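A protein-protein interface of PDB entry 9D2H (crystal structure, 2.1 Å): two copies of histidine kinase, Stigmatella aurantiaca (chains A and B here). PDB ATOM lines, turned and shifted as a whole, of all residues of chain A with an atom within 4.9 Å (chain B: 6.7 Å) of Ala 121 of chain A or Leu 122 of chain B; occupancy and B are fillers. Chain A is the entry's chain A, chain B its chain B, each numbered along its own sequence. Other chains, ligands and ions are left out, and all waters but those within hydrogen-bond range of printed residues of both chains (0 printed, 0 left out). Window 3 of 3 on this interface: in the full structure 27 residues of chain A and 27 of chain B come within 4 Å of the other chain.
Of the 11 printed residues of chain B, 5 touch a printed residue of chain A. Hydrophobic or aromatic side chains of chain B within 4 Å of the printed part of chain A: Leu 122 and Val 125. Printed residues of chain A that touch a printed residue of chain B: Glu 118, Glu 119, Ala 121 and Val 292. Hydrophobic or aromatic side chains of chain A that line the printed part of chain B: Ala 121 and Val 292. Among the printed residues, no Asp or Glu carboxylate lies within 4 Å of a Lys or Arg side-chain nitrogen of the other chain.
Among the printed residues, merely in contact across the chains: Glu 119 of chain A with Glu 118 of chain B, Ala 121 of chain A with Leu 122 of chain B, Val 292 of chain A with Val 125 of chain B and Val 292 of chain A with Arg 126 of chain B.
Glu 118 of chain A touches Glu 119 of chain B, and with the chains exchanged Glu 119 of chain A touches Glu 118 of chain B. Ala 121 of chain A touches Leu 122 of chain B, but with the chains exchanged Leu 122 of chain A does not touch Ala 121 of chain B (4.2 Å). Positions printed for both chains: 117, 118, 119, 120, 121, 122, 123, 124 and 125. Of the 5 pairs that touch across the chains among the printed residues, 2 have their exchanged pair printed and touching as well.
The side-chain carboxylate (OE2) of Glu 118 of chain A sits close to the side-chain carboxylate (OE2) of Glu 119 of chain B (3.3 Å).
The side-chain carboxylate (OE2) of Glu 123 of chain B is in salt-bridge range of the guanidinium group (NH2) of Arg 126 of chain B (3.0 Å).
Of chain B, only Leu 122 comes within 4 Å of Ala 121 of chain A. Printed residues of chain B within 4 Å of Val 292 of chain A: Val 125 (3.96 Å) and Arg 126 (3.3 Å). Printed residues of chain A within 4 Å of Glu 118 of chain B: Glu 119. Of the printed residues of chain A, Leu 122 of chain B touches Ala 121. Of the printed residues of chain A, Arg 126 of chain B touches Val 292. The nearest printed residue of chain B that does not touch Ala 121 of chain A is Glu 118 of chain B (7.3 Å).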
ATOM      1  N   MET A 117      -8.724  -3.011   9.601  1.00  0.00           N
ATOM      2  CA  MET A 117      -8.822  -4.461   9.641  1.00  0.00           C
ATOM      3  C   MET A 117     -10.223  -4.906  10.056  1.00  0.00           C
ATOM      4  O   MET A 117     -10.838  -5.741   9.387  1.00  0.00           O
ATOM      5  CB  MET A 117      -7.749  -5.011  10.582  1.00  0.00           C
ATOM      6  CG  MET A 117      -7.555  -6.529  10.524  1.00  0.00           C
ATOM      7  SD  MET A 117      -8.848  -7.475  11.405  1.00  0.00           S
ATOM      8  CE  MET A 117      -8.446  -7.079  13.109  1.00  0.00           C
ATOM      9  N   GLU A 118     -10.752  -4.356  11.155  1.00  0.00           N
ATOM     10  CA  GLU A 118     -12.014  -4.876  11.690  1.00  0.00           C
ATOM     11  C   GLU A 118     -13.198  -4.509  10.806  1.00  0.00           C
ATOM     12  O   GLU A 118     -14.194  -5.248  10.758  1.00  0.00           O
ATOM     13  CB  GLU A 118     -12.248  -4.369  13.112  1.00  0.00           C
ATOM     14  CG  GLU A 118     -11.281  -4.910  14.143  1.00  0.00           C
ATOM     15  CD  GLU A 118      -9.973  -4.137  14.207  1.00  0.00           C
ATOM     16  OE1 GLU A 118      -9.750  -3.221  13.379  1.00  0.00           O
ATOM     17  OE2 GLU A 118      -9.156  -4.455  15.096  1.00  0.00           O
ATOM     18  N   GLU A 119     -13.117  -3.380  10.101  1.00  0.00           N
ATOM     19  CA  GLU A 119     -14.147  -3.061   9.119  1.00  0.00           C
ATOM     20  C   GLU A 119     -14.177  -4.099   8.015  1.00  0.00           C
ATOM     21  O   GLU A 119     -15.244  -4.417   7.484  1.00  0.00           O
ATOM     22  CB  GLU A 119     -13.894  -1.680   8.539  1.00  0.00           C
ATOM     23  CG  GLU A 119     -14.972  -1.201   7.613  1.00  0.00           C
ATOM     24  CD  GLU A 119     -14.729   0.232   7.187  1.00  0.00           C
ATOM     25  OE1 GLU A 119     -13.608   0.731   7.464  1.00  0.00           O
ATOM     26  OE2 GLU A 119     -15.654   0.855   6.599  1.00  0.00           O
ATOM     27  N   THR A 120     -13.010  -4.643   7.670  1.00  0.00           N
ATOM     28  CA  THR A 120     -12.927  -5.681   6.648  1.00  0.00           C
ATOM     29  C   THR A 120     -13.496  -7.002   7.155  1.00  0.00           C
ATOM     30  O   THR A 120     -14.162  -7.727   6.404  1.00  0.00           O
ATOM     31  CB  THR A 120     -11.470  -5.853   6.204  1.00  0.00           C
ATOM     32  OG1 THR A 120     -10.994  -4.628   5.622  1.00  0.00           O
ATOM     33  CG2 THR A 120     -11.337  -6.982   5.207  1.00  0.00           C
ATOM     34  N   ALA A 121     -13.240  -7.337   8.425  1.00  0.00           N
ATOM     35  CA  ALA A 121     -13.843  -8.537   8.990  1.00  0.00           C
ATOM     36  C   ALA A 121     -15.358  -8.382   9.123  1.00  0.00           C
ATOM     37  O   ALA A 121     -16.115  -9.332   8.897  1.00  0.00           O
ATOM     38  CB  ALA A 121     -13.198  -8.853  10.340  1.00  0.00           C
ATOM     39  N   LEU A 122     -15.826  -7.187   9.476  1.00  0.00           N
ATOM     40  CA  LEU A 122     -17.265  -6.996   9.602  1.00  0.00           C
ATOM     41  C   LEU A 122     -17.978  -7.197   8.266  1.00  0.00           C
ATOM     42  O   LEU A 122     -19.111  -7.695   8.235  1.00  0.00           O
ATOM     43  CB  LEU A 122     -17.550  -5.608  10.166  1.00  0.00           C
ATOM     44  CG  LEU A 122     -18.924  -5.415  10.781  1.00  0.00           C
ATOM     45  CD1 LEU A 122     -19.046  -6.299  12.001  1.00  0.00           C
ATOM     46  CD2 LEU A 122     -19.092  -3.948  11.142  1.00  0.00           C
ATOM     47  N   GLU A 123     -17.343  -6.834   7.150  1.00  0.00           N
ATOM     48  CA  GLU A 123     -18.001  -7.033   5.863  1.00  0.00           C
ATOM     49  C   GLU A 123     -18.115  -8.511   5.516  1.00  0.00           C
ATOM     50  O   GLU A 123     -19.141  -8.953   4.984  1.00  0.00           O
ATOM     51  CB  GLU A 123     -17.252  -6.292   4.757  1.00  0.00           C
ATOM     52  CG  GLU A 123     -17.553  -4.803   4.702  1.00  0.00           C
ATOM     53  CD  GLU A 123     -18.988  -4.505   4.273  1.00  0.00           C
ATOM     54  OE1 GLU A 123     -19.545  -5.283   3.461  1.00  0.00           O
ATOM     55  OE2 GLU A 123     -19.559  -3.496   4.753  1.00  0.00           O
ATOM     56  N   VAL A 124     -17.064  -9.290   5.781  1.00  0.00           N
ATOM     57  CA  VAL A 124     -17.115 -10.700   5.413  1.00  0.00           C
ATOM     58  C   VAL A 124     -18.021 -11.464   6.366  1.00  0.00           C
ATOM     59  O   VAL A 124     -18.598 -12.492   5.987  1.00  0.00           O
ATOM     60  CB  VAL A 124     -15.701 -11.318   5.360  1.00  0.00           C
ATOM     61  CG1 VAL A 124     -14.900 -10.722   4.231  1.00  0.00           C
ATOM     62  CG2 VAL A 124     -14.967 -11.145   6.687  1.00  0.00           C
ATOM     63  N   VAL A 125     -18.162 -10.989   7.609  1.00  0.00           N
ATOM     64  CA  VAL A 125     -19.171 -11.542   8.512  1.00  0.00           C
ATOM     65  C   VAL A 125     -20.570 -11.378   7.923  1.00  0.00           C
ATOM     66  O   VAL A 125     -21.430 -12.254   8.084  1.00  0.00           O
ATOM     67  CB  VAL A 125     -19.059 -10.885   9.899  1.00  0.00           C
ATOM     68  CG1 VAL A 125     -20.250 -11.220  10.739  1.00  0.00           C
ATOM     69  CG2 VAL A 125     -17.801 -11.333  10.590  1.00  0.00           C
ATOM     70  N   LEU A 152      -9.754 -12.600   4.258  1.00  0.00           N
ATOM     71  CA  LEU A 152      -9.359 -11.910   5.482  1.00  0.00           C
ATOM     72  C   LEU A 152      -7.891 -12.140   5.843  1.00  0.00           C
ATOM     73  O   LEU A 152      -7.283 -11.286   6.510  1.00  0.00           O
ATOM     74  CB  LEU A 152     -10.259 -12.349   6.633  1.00  0.00           C
ATOM     75  CG  LEU A 152     -10.043 -11.558   7.918  1.00  0.00           C
ATOM     76  CD1 LEU A 152     -10.068 -10.086   7.592  1.00  0.00           C
ATOM     77  CD2 LEU A 152     -11.090 -11.893   8.963  1.00  0.00           C
ATOM     78  N   ALA A 289     -10.540 -12.485  14.373  1.00  0.00           N
ATOM     79  CA  ALA A 289     -11.593 -12.222  13.394  1.00  0.00           C
ATOM     80  C   ALA A 289     -11.954 -13.492  12.632  1.00  0.00           C
ATOM     81  O   ALA A 289     -13.135 -13.816  12.454  1.00  0.00           O
ATOM     82  CB  ALA A 289     -11.157 -11.114  12.432  1.00  0.00           C
ATOM     83  N   VAL A 292     -14.286 -15.722  14.584  1.00  0.00           N
ATOM     84  CA  VAL A 292     -15.683 -15.346  14.389  1.00  0.00           C
ATOM     85  C   VAL A 292     -16.269 -16.058  13.175  1.00  0.00           C
ATOM     86  O   VAL A 292     -17.373 -16.612  13.238  1.00  0.00           O
ATOM     87  CB  VAL A 292     -15.808 -13.815  14.263  1.00  0.00           C
ATOM     88  CG1 VAL A 292     -17.099 -13.438  13.576  1.00  0.00           C
ATOM     89  CG2 VAL A 292     -15.737 -13.158  15.628  1.00  0.00           C
ATOM     90  N   MET B 117     -15.438   2.038  15.920  1.00  0.00           N
ATOM     91  CA  MET B 117     -16.793   1.496  15.957  1.00  0.00           C
ATOM     92  C   MET B 117     -16.810   0.030  15.543  1.00  0.00           C
ATOM     93  O   MET B 117     -17.447  -0.807  16.196  1.00  0.00           O
ATOM     94  CB  MET B 117     -17.715   2.321  15.060  1.00  0.00           C
ATOM     95  CG  MET B 117     -19.193   1.918  15.147  1.00  0.00           C
ATOM     96  SD  MET B 117     -19.684   0.560  14.049  1.00  0.00           S
ATOM     97  CE  MET B 117     -19.470   1.316  12.424  1.00  0.00           C
ATOM     98  N   GLU B 118     -16.132  -0.295  14.443  1.00  0.00           N
ATOM     99  CA  GLU B 118     -16.191  -1.655  13.923  1.00  0.00           C
ATOM    100  C   GLU B 118     -15.470  -2.637  14.844  1.00  0.00           C
ATOM    101  O   GLU B 118     -15.868  -3.804  14.944  1.00  0.00           O
ATOM    102  CB  GLU B 118     -15.612  -1.685  12.510  1.00  0.00           C
ATOM    103  CG  GLU B 118     -16.441  -0.929  11.469  1.00  0.00           C
ATOM    104  CD  GLU B 118     -16.159   0.573  11.414  1.00  0.00           C
ATOM    105  OE1 GLU B 118     -15.311   1.081  12.184  1.00  0.00           O
ATOM    106  OE2 GLU B 118     -16.795   1.257  10.581  1.00  0.00           O
ATOM    107  N   GLU B 119     -14.430  -2.180  15.545  1.00  0.00           N
ATOM    108  CA  GLU B 119     -13.776  -3.029  16.538  1.00  0.00           C
ATOM    109  C   GLU B 119     -14.742  -3.401  17.653  1.00  0.00           C
ATOM    110  O   GLU B 119     -14.847  -4.571  18.039  1.00  0.00           O
ATOM    111  CB  GLU B 119     -12.555  -2.327  17.110  1.00  0.00           C
ATOM    112  CG  GLU B 119     -11.587  -3.254  17.798  1.00  0.00           C
ATOM    113  CD  GLU B 119     -10.309  -2.535  18.188  1.00  0.00           C
ATOM    114  OE1 GLU B 119     -10.413  -1.337  18.544  1.00  0.00           O
ATOM    115  OE2 GLU B 119      -9.212  -3.153  18.123  1.00  0.00           O
ATOM    116  N   THR B 120     -15.459  -2.413  18.189  1.00  0.00           N
ATOM    117  CA  THR B 120     -16.463  -2.725  19.199  1.00  0.00           C
ATOM    118  C   THR B 120     -17.616  -3.526  18.599  1.00  0.00           C
ATOM    119  O   THR B 120     -18.191  -4.391  19.273  1.00  0.00           O
ATOM    120  CB  THR B 120     -16.979  -1.441  19.846  1.00  0.00           C
ATOM    121  OG1 THR B 120     -15.892  -0.537  20.061  1.00  0.00           O
ATOM    122  CG2 THR B 120     -17.588  -1.751  21.175  1.00  0.00           C
ATOM    123  N   ALA B 121     -17.974  -3.250  17.343  1.00  0.00           N
ATOM    124  CA  ALA B 121     -18.981  -4.058  16.673  1.00  0.00           C
ATOM    125  C   ALA B 121     -18.550  -5.521  16.624  1.00  0.00           C
ATOM    126  O   ALA B 121     -19.334  -6.424  16.935  1.00  0.00           O
ATOM    127  CB  ALA B 121     -19.229  -3.514  15.268  1.00  0.00           C
ATOM    128  N   LEU B 122     -17.294  -5.775  16.270  1.00  0.00           N
ATOM    129  CA  LEU B 122     -16.832  -7.154  16.184  1.00  0.00           C
ATOM    130  C   LEU B 122     -16.847  -7.840  17.549  1.00  0.00           C
ATOM    131  O   LEU B 122     -17.080  -9.054  17.635  1.00  0.00           O
ATOM    132  CB  LEU B 122     -15.436  -7.181  15.561  1.00  0.00           C
ATOM    133  CG  LEU B 122     -14.964  -8.457  14.881  1.00  0.00           C
ATOM    134  CD1 LEU B 122     -16.033  -8.985  13.948  1.00  0.00           C
ATOM    135  CD2 LEU B 122     -13.706  -8.130  14.117  1.00  0.00           C
ATOM    136  N   GLU B 123     -16.649  -7.080  18.629  1.00  0.00           N
ATOM    137  CA  GLU B 123     -16.634  -7.686  19.958  1.00  0.00           C
ATOM    138  C   GLU B 123     -18.022  -8.158  20.383  1.00  0.00           C
ATOM    139  O   GLU B 123     -18.170  -9.270  20.905  1.00  0.00           O
ATOM    140  CB  GLU B 123     -16.058  -6.708  20.986  1.00  0.00           C
ATOM    141  CG  GLU B 123     -14.536  -6.766  21.080  1.00  0.00           C
ATOM    142  CD  GLU B 123     -14.013  -8.203  21.120  1.00  0.00           C
ATOM    143  OE1 GLU B 123     -14.322  -8.926  22.099  1.00  0.00           O
ATOM    144  OE2 GLU B 123     -13.313  -8.612  20.158  1.00  0.00           O
ATOM    145  N   VAL B 124     -19.049  -7.317  20.205  1.00  0.00           N
ATOM    146  CA  VAL B 124     -20.402  -7.758  20.545  1.00  0.00           C
ATOM    147  C   VAL B 124     -20.831  -8.912  19.641  1.00  0.00           C
ATOM    148  O   VAL B 124     -21.548  -9.816  20.088  1.00  0.00           O
ATOM    149  CB  VAL B 124     -21.423  -6.594  20.492  1.00  0.00           C
ATOM    150  CG1 VAL B 124     -21.272  -5.684  21.673  1.00  0.00           C
ATOM    151  CG2 VAL B 124     -21.292  -5.785  19.218  1.00  0.00           C
ATOM    152  N   VAL B 125     -20.404  -8.911  18.372  1.00  0.00           N
ATOM    153  CA  VAL B 125     -20.698 -10.036  17.483  1.00  0.00           C
ATOM    154  C   VAL B 125     -20.187 -11.342  18.082  1.00  0.00           C
ATOM    155  O   VAL B 125     -20.879 -12.371  18.050  1.00  0.00           O
ATOM    156  CB  VAL B 125     -20.108  -9.778  16.084  1.00  0.00           C
ATOM    157  CG1 VAL B 125     -19.708 -11.089  15.403  1.00  0.00           C
ATOM    158  CG2 VAL B 125     -21.119  -9.040  15.248  1.00  0.00           C
ATOM    159  N   ARG B 126     -18.975 -11.312  18.652  1.00  0.00           N
ATOM    160  CA  ARG B 126     -18.422 -12.470  19.347  1.00  0.00           C
ATOM    161  C   ARG B 126     -19.336 -12.925  20.480  1.00  0.00           C
ATOM    162  O   ARG B 126     -19.502 -14.130  20.717  1.00  0.00           O
ATOM    163  CB  ARG B 126     -17.031 -12.125  19.889  1.00  0.00           C
ATOM    164  CG  ARG B 126     -16.042 -13.284  19.892  1.00  0.00           C
ATOM    165  CD  ARG B 126     -14.658 -12.848  20.362  1.00  0.00           C
ATOM    166  NE  ARG B 126     -14.177 -11.681  19.630  1.00  0.00           N
ATOM    167  CZ  ARG B 126     -13.554 -11.736  18.460  1.00  0.00           C
ATOM    168  NH1 ARG B 126     -13.328 -12.894  17.849  1.00  0.00           N
ATOM    169  NH2 ARG B 126     -13.149 -10.602  17.887  1.00  0.00           N
ATOM    170  N   ARG B 127     -19.934 -11.969  21.195  1.00  0.00           N
ATOM    171  CA  ARG B 127     -20.810 -12.291  22.312  1.00  0.00           C
ATOM    172  C   ARG B 127     -22.090 -12.993  21.868  1.00  0.00           C
ATOM    173  O   ARG B 127     -22.686 -13.738  22.656  1.00  0.00           O
ATOM    174  CB  ARG B 127     -21.129 -11.005  23.072  1.00  0.00           C
ATOM    175  CG  ARG B 127     -21.790 -11.208  24.409  1.00  0.00           C
ATOM    176  CD  ARG B 127     -22.002  -9.876  25.134  1.00  0.00           C
ATOM    177  NE  ARG B 127     -21.794 -10.027  26.572  1.00  0.00           N
ATOM    178  CZ  ARG B 127     -22.151  -9.140  27.491  1.00  0.00           C
ATOM    179  NH1 ARG B 127     -22.778  -8.018  27.166  1.00  0.00           N
ATOM    180  NH2 ARG B 127     -21.878  -9.386  28.772  1.00  0.00           N
